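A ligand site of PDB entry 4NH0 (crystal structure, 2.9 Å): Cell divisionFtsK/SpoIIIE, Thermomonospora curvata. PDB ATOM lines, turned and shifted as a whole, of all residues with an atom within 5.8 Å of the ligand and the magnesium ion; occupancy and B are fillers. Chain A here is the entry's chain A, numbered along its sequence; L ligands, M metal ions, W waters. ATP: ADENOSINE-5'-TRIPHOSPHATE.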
ATOM      1  N   ASN A 905      -2.866 -24.300   5.676  1.00  0.00           N
ATOM      2  CA  ASN A 905      -1.605 -23.863   6.237  1.00  0.00           C
ATOM      3  C   ASN A 905      -0.856 -25.062   6.797  1.00  0.00           C
ATOM      4  O   ASN A 905       0.370 -25.135   6.748  1.00  0.00           O
ATOM      5  CB  ASN A 905      -1.818 -22.808   7.324  1.00  0.00           C
ATOM      6  CG  ASN A 905      -2.258 -21.477   6.770  1.00  0.00           C
ATOM      7  OD1 ASN A 905      -1.832 -21.078   5.679  1.00  0.00           O
ATOM      8  ND2 ASN A 905      -3.118 -20.779   7.494  1.00  0.00           N
ATOM      9  N   VAL A 906      -1.619 -26.020   7.329  1.00  0.00           N
ATOM     10  CA  VAL A 906      -1.062 -27.271   7.813  1.00  0.00           C
ATOM     11  C   VAL A 906      -1.929 -28.442   7.345  1.00  0.00           C
ATOM     12  O   VAL A 906      -3.126 -28.490   7.643  1.00  0.00           O
ATOM     13  CB  VAL A 906      -0.936 -27.286   9.343  1.00  0.00           C
ATOM     14  CG1 VAL A 906      -2.163 -26.683  10.005  1.00  0.00           C
ATOM     15  CG2 VAL A 906      -0.677 -28.700   9.846  1.00  0.00           C
ATOM     16  N   LEU A 907      -1.331 -29.366   6.609  1.00  0.00           N
ATOM     17  CA  LEU A 907      -2.035 -30.533   6.128  1.00  0.00           C
ATOM     18  C   LEU A 907      -1.582 -31.776   6.882  1.00  0.00           C
ATOM     19  O   LEU A 907      -0.430 -32.187   6.766  1.00  0.00           O
ATOM     20  CB  LEU A 907      -1.816 -30.725   4.628  1.00  0.00           C
ATOM     21  CG  LEU A 907      -2.370 -32.010   4.012  1.00  0.00           C
ATOM     22  CD1 LEU A 907      -3.881 -32.046   4.141  1.00  0.00           C
ATOM     23  CD2 LEU A 907      -1.957 -32.139   2.557  1.00  0.00           C
ATOM     24  N   ASP A 949      14.565 -23.300   1.627  1.00  0.00           N
ATOM     25  CA  ASP A 949      15.334 -22.525   2.595  1.00  0.00           C
ATOM     26  C   ASP A 949      15.227 -23.082   4.004  1.00  0.00           C
ATOM     27  O   ASP A 949      14.606 -24.126   4.222  1.00  0.00           O
ATOM     28  CB  ASP A 949      14.899 -21.052   2.576  1.00  0.00           C
ATOM     29  CG  ASP A 949      13.394 -20.880   2.725  1.00  0.00           C
ATOM     30  OD1 ASP A 949      12.788 -21.553   3.589  1.00  0.00           O
ATOM     31  OD2 ASP A 949      12.817 -20.063   1.986  1.00  0.00           O
ATOM     32  N   THR A 950      15.826 -22.396   4.964  1.00  0.00           N
ATOM     33  CA  THR A 950      15.816 -22.832   6.350  1.00  0.00           C
ATOM     34  C   THR A 950      14.413 -22.811   6.932  1.00  0.00           C
ATOM     35  O   THR A 950      13.678 -21.832   6.757  1.00  0.00           O
ATOM     36  CB  THR A 950      16.735 -21.957   7.225  1.00  0.00           C
ATOM     37  OG1 THR A 950      16.366 -20.583   7.075  1.00  0.00           O
ATOM     38  CG2 THR A 950      18.187 -22.129   6.801  1.00  0.00           C
ATOM     39  N   GLU A 951      14.045 -23.897   7.610  1.00  0.00           N
ATOM     40  CA  GLU A 951      12.734 -24.048   8.229  1.00  0.00           C
ATOM     41  C   GLU A 951      11.599 -23.847   7.230  1.00  0.00           C
ATOM     42  O   GLU A 951      10.794 -22.934   7.376  1.00  0.00           O
ATOM     43  CB  GLU A 951      12.571 -23.065   9.399  1.00  0.00           C
ATOM     44  CG  GLU A 951      13.570 -23.284  10.532  1.00  0.00           C
ATOM     45  CD  GLU A 951      13.262 -22.430  11.735  1.00  0.00           C
ATOM     46  OE1 GLU A 951      12.110 -21.960  11.855  1.00  0.00           O
ATOM     47  OE2 GLU A 951      14.173 -22.221  12.567  1.00  0.00           O
ATOM     48  N   CYS A 952      11.552 -24.707   6.217  1.00  0.00           N
ATOM     49  CA  CYS A 952      10.488 -24.658   5.226  1.00  0.00           C
ATOM     50  C   CYS A 952       9.688 -25.950   5.248  1.00  0.00           C
ATOM     51  O   CYS A 952       8.494 -25.963   4.958  1.00  0.00           O
ATOM     52  CB  CYS A 952      11.049 -24.404   3.833  1.00  0.00           C
ATOM     53  SG  CYS A 952      12.004 -25.781   3.161  1.00  0.00           S
ATOM     54  N   GLY A 953      10.354 -27.052   5.586  1.00  0.00           N
ATOM     55  CA  GLY A 953       9.692 -28.334   5.686  1.00  0.00           C
ATOM     56  C   GLY A 953      10.434 -29.466   5.006  1.00  0.00           C
ATOM     57  O   GLY A 953       9.827 -30.463   4.603  1.00  0.00           O
ATOM     58  N   LYS A 954      11.759 -29.316   4.880  1.00  0.00           N
ATOM     59  CA  LYS A 954      12.573 -30.348   4.237  1.00  0.00           C
ATOM     60  C   LYS A 954      12.599 -31.630   5.053  1.00  0.00           C
ATOM     61  O   LYS A 954      12.165 -32.680   4.580  1.00  0.00           O
ATOM     62  CB  LYS A 954      13.996 -29.842   4.004  1.00  0.00           C
ATOM     63  CG  LYS A 954      14.117 -28.707   3.008  1.00  0.00           C
ATOM     64  CD  LYS A 954      15.477 -28.033   3.083  1.00  0.00           C
ATOM     65  CE  LYS A 954      15.485 -26.903   4.099  1.00  0.00           C
ATOM     66  NZ  LYS A 954      15.751 -27.376   5.483  1.00  0.00           N
ATOM     67  N   SER A 955      13.112 -31.547   6.271  1.00  0.00           N
ATOM     68  CA  SER A 955      13.253 -32.708   7.149  1.00  0.00           C
ATOM     69  C   SER A 955      11.919 -33.413   7.388  1.00  0.00           C
ATOM     70  O   SER A 955      11.873 -34.639   7.464  1.00  0.00           O
ATOM     71  CB  SER A 955      13.871 -32.294   8.481  1.00  0.00           C
ATOM     72  OG  SER A 955      15.112 -31.653   8.290  1.00  0.00           O
ATOM     73  N   ASN A 956      10.855 -32.640   7.506  1.00  0.00           N
ATOM     74  CA  ASN A 956       9.525 -33.198   7.697  1.00  0.00           C
ATOM     75  C   ASN A 956       9.072 -34.017   6.503  1.00  0.00           C
ATOM     76  O   ASN A 956       8.515 -35.102   6.645  1.00  0.00           O
ATOM     77  CB  ASN A 956       8.510 -32.086   7.966  1.00  0.00           C
ATOM     78  CG  ASN A 956       7.085 -32.602   8.027  1.00  0.00           C
ATOM     79  OD1 ASN A 956       6.620 -33.075   9.065  1.00  0.00           O
ATOM     80  ND2 ASN A 956       6.383 -32.516   6.905  1.00  0.00           N
ATOM     81  N   LEU A 957       9.317 -33.482   5.301  1.00  0.00           N
ATOM     82  CA  LEU A 957       8.956 -34.170   4.070  1.00  0.00           C
ATOM     83  C   LEU A 957       9.761 -35.462   3.932  1.00  0.00           C
ATOM     84  O   LEU A 957       9.257 -36.459   3.418  1.00  0.00           O
ATOM     85  CB  LEU A 957       9.194 -33.273   2.864  1.00  0.00           C
ATOM     86  CG  LEU A 957       9.012 -33.906   1.485  1.00  0.00           C
ATOM     87  CD1 LEU A 957       7.596 -34.422   1.326  1.00  0.00           C
ATOM     88  CD2 LEU A 957       9.350 -32.928   0.393  1.00  0.00           C
ATOM     89  N   ARG A 959      10.899 -37.338   6.415  1.00  0.00           N
ATOM     90  CA  ARG A 959      10.342 -38.303   7.358  1.00  0.00           C
ATOM     91  C   ARG A 959       9.004 -38.830   6.846  1.00  0.00           C
ATOM     92  O   ARG A 959       8.664 -39.989   7.068  1.00  0.00           O
ATOM     93  CB  ARG A 959      10.198 -37.688   8.742  1.00  0.00           C
ATOM     94  CG  ARG A 959      11.511 -37.515   9.479  1.00  0.00           C
ATOM     95  CD  ARG A 959      11.323 -36.971  10.891  1.00  0.00           C
ATOM     96  NE  ARG A 959      11.272 -35.512  10.913  1.00  0.00           N
ATOM     97  CZ  ARG A 959      10.187 -34.802  11.184  1.00  0.00           C
ATOM     98  NH1 ARG A 959       9.041 -35.418  11.464  1.00  0.00           N
ATOM     99  NH2 ARG A 959      10.240 -33.476  11.191  1.00  0.00           N
ATOM    100  N   SER A 984      18.102 -35.366  12.232  1.00  0.00           N
ATOM    101  CA  SER A 984      16.707 -34.934  12.238  1.00  0.00           C
ATOM    102  C   SER A 984      15.783 -36.107  11.954  1.00  0.00           C
ATOM    103  O   SER A 984      14.569 -35.996  12.052  1.00  0.00           O
ATOM    104  CB  SER A 984      16.494 -33.833  11.201  1.00  0.00           C
ATOM    105  OG  SER A 984      17.078 -32.609  11.597  1.00  0.00           O
ATOM    106  N   ASP A1045      19.623 -36.111   4.044  1.00  0.00           N
ATOM    107  CA  ASP A1045      19.107 -34.823   4.492  1.00  0.00           C
ATOM    108  C   ASP A1045      20.262 -33.827   4.624  1.00  0.00           C
ATOM    109  O   ASP A1045      21.384 -34.219   4.953  1.00  0.00           O
ATOM    110  CB  ASP A1045      18.383 -34.973   5.836  1.00  0.00           C
ATOM    111  CG  ASP A1045      17.485 -33.787   6.146  1.00  0.00           C
ATOM    112  OD1 ASP A1045      17.638 -32.726   5.506  1.00  0.00           O
ATOM    113  OD2 ASP A1045      16.615 -33.916   7.030  1.00  0.00           O
ATOM    114  N   ASP A1046      19.972 -32.561   4.356  1.00  0.00           N
ATOM    115  CA  ASP A1046      20.973 -31.502   4.393  1.00  0.00           C
ATOM    116  C   ASP A1046      22.161 -31.827   3.485  1.00  0.00           C
ATOM    117  O   ASP A1046      23.281 -32.010   3.952  1.00  0.00           O
ATOM    118  CB  ASP A1046      21.453 -31.251   5.819  1.00  0.00           C
ATOM    119  CG  ASP A1046      20.345 -30.792   6.734  1.00  0.00           C
ATOM    120  OD1 ASP A1046      19.589 -29.877   6.341  1.00  0.00           O
ATOM    121  OD2 ASP A1046      20.210 -31.344   7.848  1.00  0.00           O
ATOM    122  N   GLN A1125       5.373 -22.490   4.983  1.00  0.00           N
ATOM    123  CA  GLN A1125       5.954 -23.775   5.346  1.00  0.00           C
ATOM    124  C   GLN A1125       5.182 -24.946   4.731  1.00  0.00           C
ATOM    125  O   GLN A1125       3.955 -24.984   4.778  1.00  0.00           O
ATOM    126  CB  GLN A1125       6.000 -23.924   6.869  1.00  0.00           C
ATOM    127  CG  GLN A1125       6.889 -22.914   7.558  1.00  0.00           C
ATOM    128  CD  GLN A1125       6.940 -23.110   9.060  1.00  0.00           C
ATOM    129  OE1 GLN A1125       5.943 -23.507   9.677  1.00  0.00           O
ATOM    130  NE2 GLN A1125       8.092 -22.830   9.659  1.00  0.00           N
ATOM    131  N   GLY A1126       5.921 -25.888   4.164  1.00  0.00           N
ATOM    132  CA  GLY A1126       5.321 -27.089   3.600  1.00  0.00           C
ATOM    133  C   GLY A1126       4.959 -26.962   2.139  1.00  0.00           C
ATOM    134  O   GLY A1126       4.881 -27.954   1.424  1.00  0.00           O
ATOM    135  N   GLN A1141       0.862 -28.634  -1.656  1.00  0.00           N
ATOM    136  CA  GLN A1141       1.095 -28.443  -0.229  1.00  0.00           C
ATOM    137  C   GLN A1141       1.431 -29.784   0.416  1.00  0.00           C
ATOM    138  O   GLN A1141       0.624 -30.706   0.388  1.00  0.00           O
ATOM    139  CB  GLN A1141      -0.123 -27.814   0.448  1.00  0.00           C
ATOM    140  CG  GLN A1141      -0.053 -27.821   1.965  1.00  0.00           C
ATOM    141  CD  GLN A1141       0.843 -26.728   2.507  1.00  0.00           C
ATOM    142  OE1 GLN A1141       1.044 -25.701   1.866  1.00  0.00           O
ATOM    143  NE2 GLN A1141       1.387 -26.948   3.700  1.00  0.00           N
ATOM    144  N   THR A1142       2.628 -29.895   0.974  1.00  0.00           N
ATOM    145  CA  THR A1142       3.065 -31.146   1.587  1.00  0.00           C
ATOM    146  C   THR A1142       2.416 -31.351   2.942  1.00  0.00           C
ATOM    147  O   THR A1142       1.970 -30.401   3.583  1.00  0.00           O
ATOM    148  CB  THR A1142       4.586 -31.201   1.734  1.00  0.00           C
ATOM    149  OG1 THR A1142       5.047 -30.072   2.472  1.00  0.00           O
ATOM    150  CG2 THR A1142       5.253 -31.204   0.375  1.00  0.00           C
ATOM    151  N   ALA A1143       2.366 -32.605   3.395  1.00  0.00           N
ATOM    152  CA  ALA A1143       1.689 -32.950   4.634  1.00  0.00           C
ATOM    153  C   ALA A1143       2.608 -32.890   5.841  1.00  0.00           C
ATOM    154  O   ALA A1143       3.805 -33.137   5.740  1.00  0.00           O
ATOM    155  CB  ALA A1143       1.075 -34.331   4.518  1.00  0.00           C
ATOM    156  N   TYR A1144       2.034 -32.546   6.994  1.00  0.00           N
ATOM    157  CA  TYR A1144       2.793 -32.437   8.225  1.00  0.00           C
ATOM    158  C   TYR A1144       2.698 -33.713   9.060  1.00  0.00           C
ATOM    159  O   TYR A1144       1.608 -34.237   9.285  1.00  0.00           O
ATOM    160  CB  TYR A1144       2.295 -31.239   9.049  1.00  0.00           C
ATOM    161  CG  TYR A1144       2.968 -31.096  10.398  1.00  0.00           C
ATOM    162  CD1 TYR A1144       4.292 -30.703  10.499  1.00  0.00           C
ATOM    163  CD2 TYR A1144       2.270 -31.353  11.567  1.00  0.00           C
ATOM    164  CE1 TYR A1144       4.902 -30.575  11.729  1.00  0.00           C
ATOM    165  CE2 TYR A1144       2.871 -31.219  12.805  1.00  0.00           C
ATOM    166  CZ  TYR A1144       4.191 -30.830  12.878  1.00  0.00           C
ATOM    167  OH  TYR A1144       4.799 -30.697  14.101  1.00  0.00           O
ATOM    168  N   ARG A1145       3.851 -34.216   9.490  1.00  0.00           N
ATOM    169  CA  ARG A1145       3.912 -35.444  10.269  1.00  0.00           C
ATOM    170  C   ARG A1145       4.478 -35.187  11.659  1.00  0.00           C
ATOM    171  O   ARG A1145       5.652 -34.877  11.813  1.00  0.00           O
ATOM    172  CB  ARG A1145       4.763 -36.488   9.542  1.00  0.00           C
ATOM    173  CG  ARG A1145       4.957 -37.776  10.310  1.00  0.00           C
ATOM    174  CD  ARG A1145       5.828 -38.749   9.538  1.00  0.00           C
ATOM    175  NE  ARG A1145       6.015 -40.012  10.238  1.00  0.00           N
ATOM    176  CZ  ARG A1145       6.939 -40.226  11.157  1.00  0.00           C
ATOM    177  NH1 ARG A1145       7.778 -39.261  11.498  1.00  0.00           N
ATOM    178  NH2 ARG A1145       7.039 -41.414  11.748  1.00  0.00           N
HETATM  179  PG  ATP L   1      16.086 -26.778   8.930  1.00  0.00           P
HETATM  180  O1G ATP L   1      15.751 -27.332  10.288  1.00  0.00           O
HETATM  181  O2G ATP L   1      16.600 -25.360   8.940  1.00  0.00           O
HETATM  182  O3G ATP L   1      16.871 -27.723   8.065  1.00  0.00           O
HETATM  183  PB  ATP L   1      13.755 -27.979   7.993  1.00  0.00           P
HETATM  184  O1B ATP L   1      14.350 -29.130   8.766  1.00  0.00           O
HETATM  185  O2B ATP L   1      13.484 -28.134   6.515  1.00  0.00           O
HETATM  186  O3B ATP L   1      14.657 -26.670   8.191  1.00  0.00           O
HETATM  187  PA  ATP L   1      11.458 -28.709   9.375  1.00  0.00           P
HETATM  188  O1A ATP L   1      10.960 -29.651   8.312  1.00  0.00           O
HETATM  189  O2A ATP L   1      12.236 -29.262  10.544  1.00  0.00           O
HETATM  190  O3A ATP L   1      12.349 -27.574   8.660  1.00  0.00           O
HETATM  191  O5' ATP L   1      10.218 -27.868   9.931  1.00  0.00           O
HETATM  192  C5' ATP L   1      10.408 -26.606  10.574  1.00  0.00           C
HETATM  193  C4' ATP L   1       9.045 -26.064  10.956  1.00  0.00           C
HETATM  194  O4' ATP L   1       8.198 -26.064   9.807  1.00  0.00           O
HETATM  195  C3' ATP L   1       8.380 -26.935  12.016  1.00  0.00           C
HETATM  196  O3' ATP L   1       8.207 -26.190  13.223  1.00  0.00           O
HETATM  197  C2' ATP L   1       7.027 -27.326  11.455  1.00  0.00           C
HETATM  198  O2' ATP L   1       5.994 -26.871  12.329  1.00  0.00           O
HETATM  199  C1' ATP L   1       6.922 -26.624  10.106  1.00  0.00           C
HETATM  200  N9  ATP L   1       6.544 -27.590   9.050  1.00  0.00           N
HETATM  201  C8  ATP L   1       7.320 -28.577   8.579  1.00  0.00           C
HETATM  202  N7  ATP L   1       6.686 -29.292   7.622  1.00  0.00           N
HETATM  203  C5  ATP L   1       5.458 -28.760   7.468  1.00  0.00           C
HETATM  204  C6  ATP L   1       4.275 -29.030   6.618  1.00  0.00           C
HETATM  205  N6  ATP L   1       4.279 -30.045   5.718  1.00  0.00           N
HETATM  206  N1  ATP L   1       3.196 -28.247   6.773  1.00  0.00           N
HETATM  207  C2  ATP L   1       3.190 -27.234   7.659  1.00  0.00           C
HETATM  208  N3  ATP L   1       4.221 -26.931   8.455  1.00  0.00           N
HETATM  209  C4  ATP L   1       5.373 -27.646   8.414  1.00  0.00           C
HETATM  210 MG    MG M   1      16.146 -29.668   8.218  1.00  0.00          MG
HETATM  211  O   HOH W   1      16.531 -30.954   6.730  1.00  0.00           O
HETATM  212  O   HOH W   2      16.172 -30.587  10.010  1.00  0.00           O
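An oxygen (O1B) of the ligand is bound to the magnesium ion, 2.0 Å away. The magnesium ion is bound by water W1 (2.0 Å). The magnesium ion is bound by water W2, at 2.0 Å. The magnesium ion is bound by O3G of the ligand, at 2.1 Å. The magnesium ion is bound by the side-chain hydroxyl (OG) of Ser 955, 2.2 Å away.
The side-chain carboxylate (OD2) of Asp 1045 sits close to the side-chain hydroxyl (OG) of Ser 955. ND2 of Asn 956 is in hydrogen-bond range of O of Ala 1143 (2.9 Å). N of Arg 1145 is in hydrogen-bond range of OD1 of Asn 956, at 3.0 Å. O of Gly 1126 lies within hydrogen-bond range of N of Thr 1142, at 3.0 Å. NE2 of Gln 1141 is in hydrogen-bond range of O of Gln 1125, at 3.4 Å. O of Leu 907 is in hydrogen-bond range of N of Tyr 1144. O of Cys 952 lies within hydrogen-bond range of N of Gly 1126, at 2.7 Å. The side-chain sulfur of Cys 952 sits at hydrogen-bond distance from the backbone carbonyl oxygen of Asp 949 (3.3 Å).
An oxygen (O2B) of the ligand lies within hydrogen-bond range of the backbone NH (N) of Ser 955, at 3.4 Å. The backbone NH (N) of Lys 954 sits at hydrogen-bond distance from an oxygen (O2B) of the ligand, 2.7 Å away. An oxygen (O2B) of the ligand is in salt-bridge range of the side-chain amino group (NZ) of Lys 954 (2.6 Å). N of Glu 951 lies within hydrogen-bond range of O3B of the ligand (2.9 Å). O1A of the ligand lies within hydrogen-bond range of N of Asn 956, 3.1 Å away. The side-chain amide nitrogen of Asn 956 lies within hydrogen-bond range of a nitrogen (N7) of the ligand (3.3 Å). O of Ala 1143 lies within hydrogen-bond range of N6 of the ligand, 3.1 Å away. N6 of the ligand sits at hydrogen-bond distance from O of Thr 1142, 3.2 Å away. N6 of the ligand is in hydrogen-bond range of OG1 of Thr 1142, 3.3 Å away. The backbone NH of Gly 953 lies within hydrogen-bond range of an oxygen (O2B) of the ligand (3.4 Å). NE2 of Gln 1125 lies within hydrogen-bond range of O4' of the ligand.
Lys 954 touches the magnesium ion (NZ to MG, 3.6 Å). Asp 1046 touches the magnesium ion (OD1 to MG, 3.9 Å). Of the 23 residues printed, 3 come within 4 Å of the magnesium ion. The nearest printed residue that does not touch the magnesium ion is Asp 1045 (4.4 Å).
O of Asn 905 touches C2 of the ligand, 3.6 Å away. Thr 950 touches the ligand. Cys 952 touches the ligand. Asp 1046 touches the ligand. Gly 1126 touches the ligand (CA to C6, 3.7 Å). Gln 1141 touches the ligand (NE2 to N1, 3.8 Å). N of Tyr 1144 touches N6 of the ligand, 3.6 Å away. Hydrophobic or aromatic side chains within 4 Å of the ligand: Tyr 1144.
Water W1 lies within hydrogen-bond range of OD1 of Asp 1045, OD1 of Asp 1046 and N of Ser 955. Water W2 lies within hydrogen-bond range of OG of Ser 984 (2.7 Å) and O1G of the ligand (3.3 Å).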
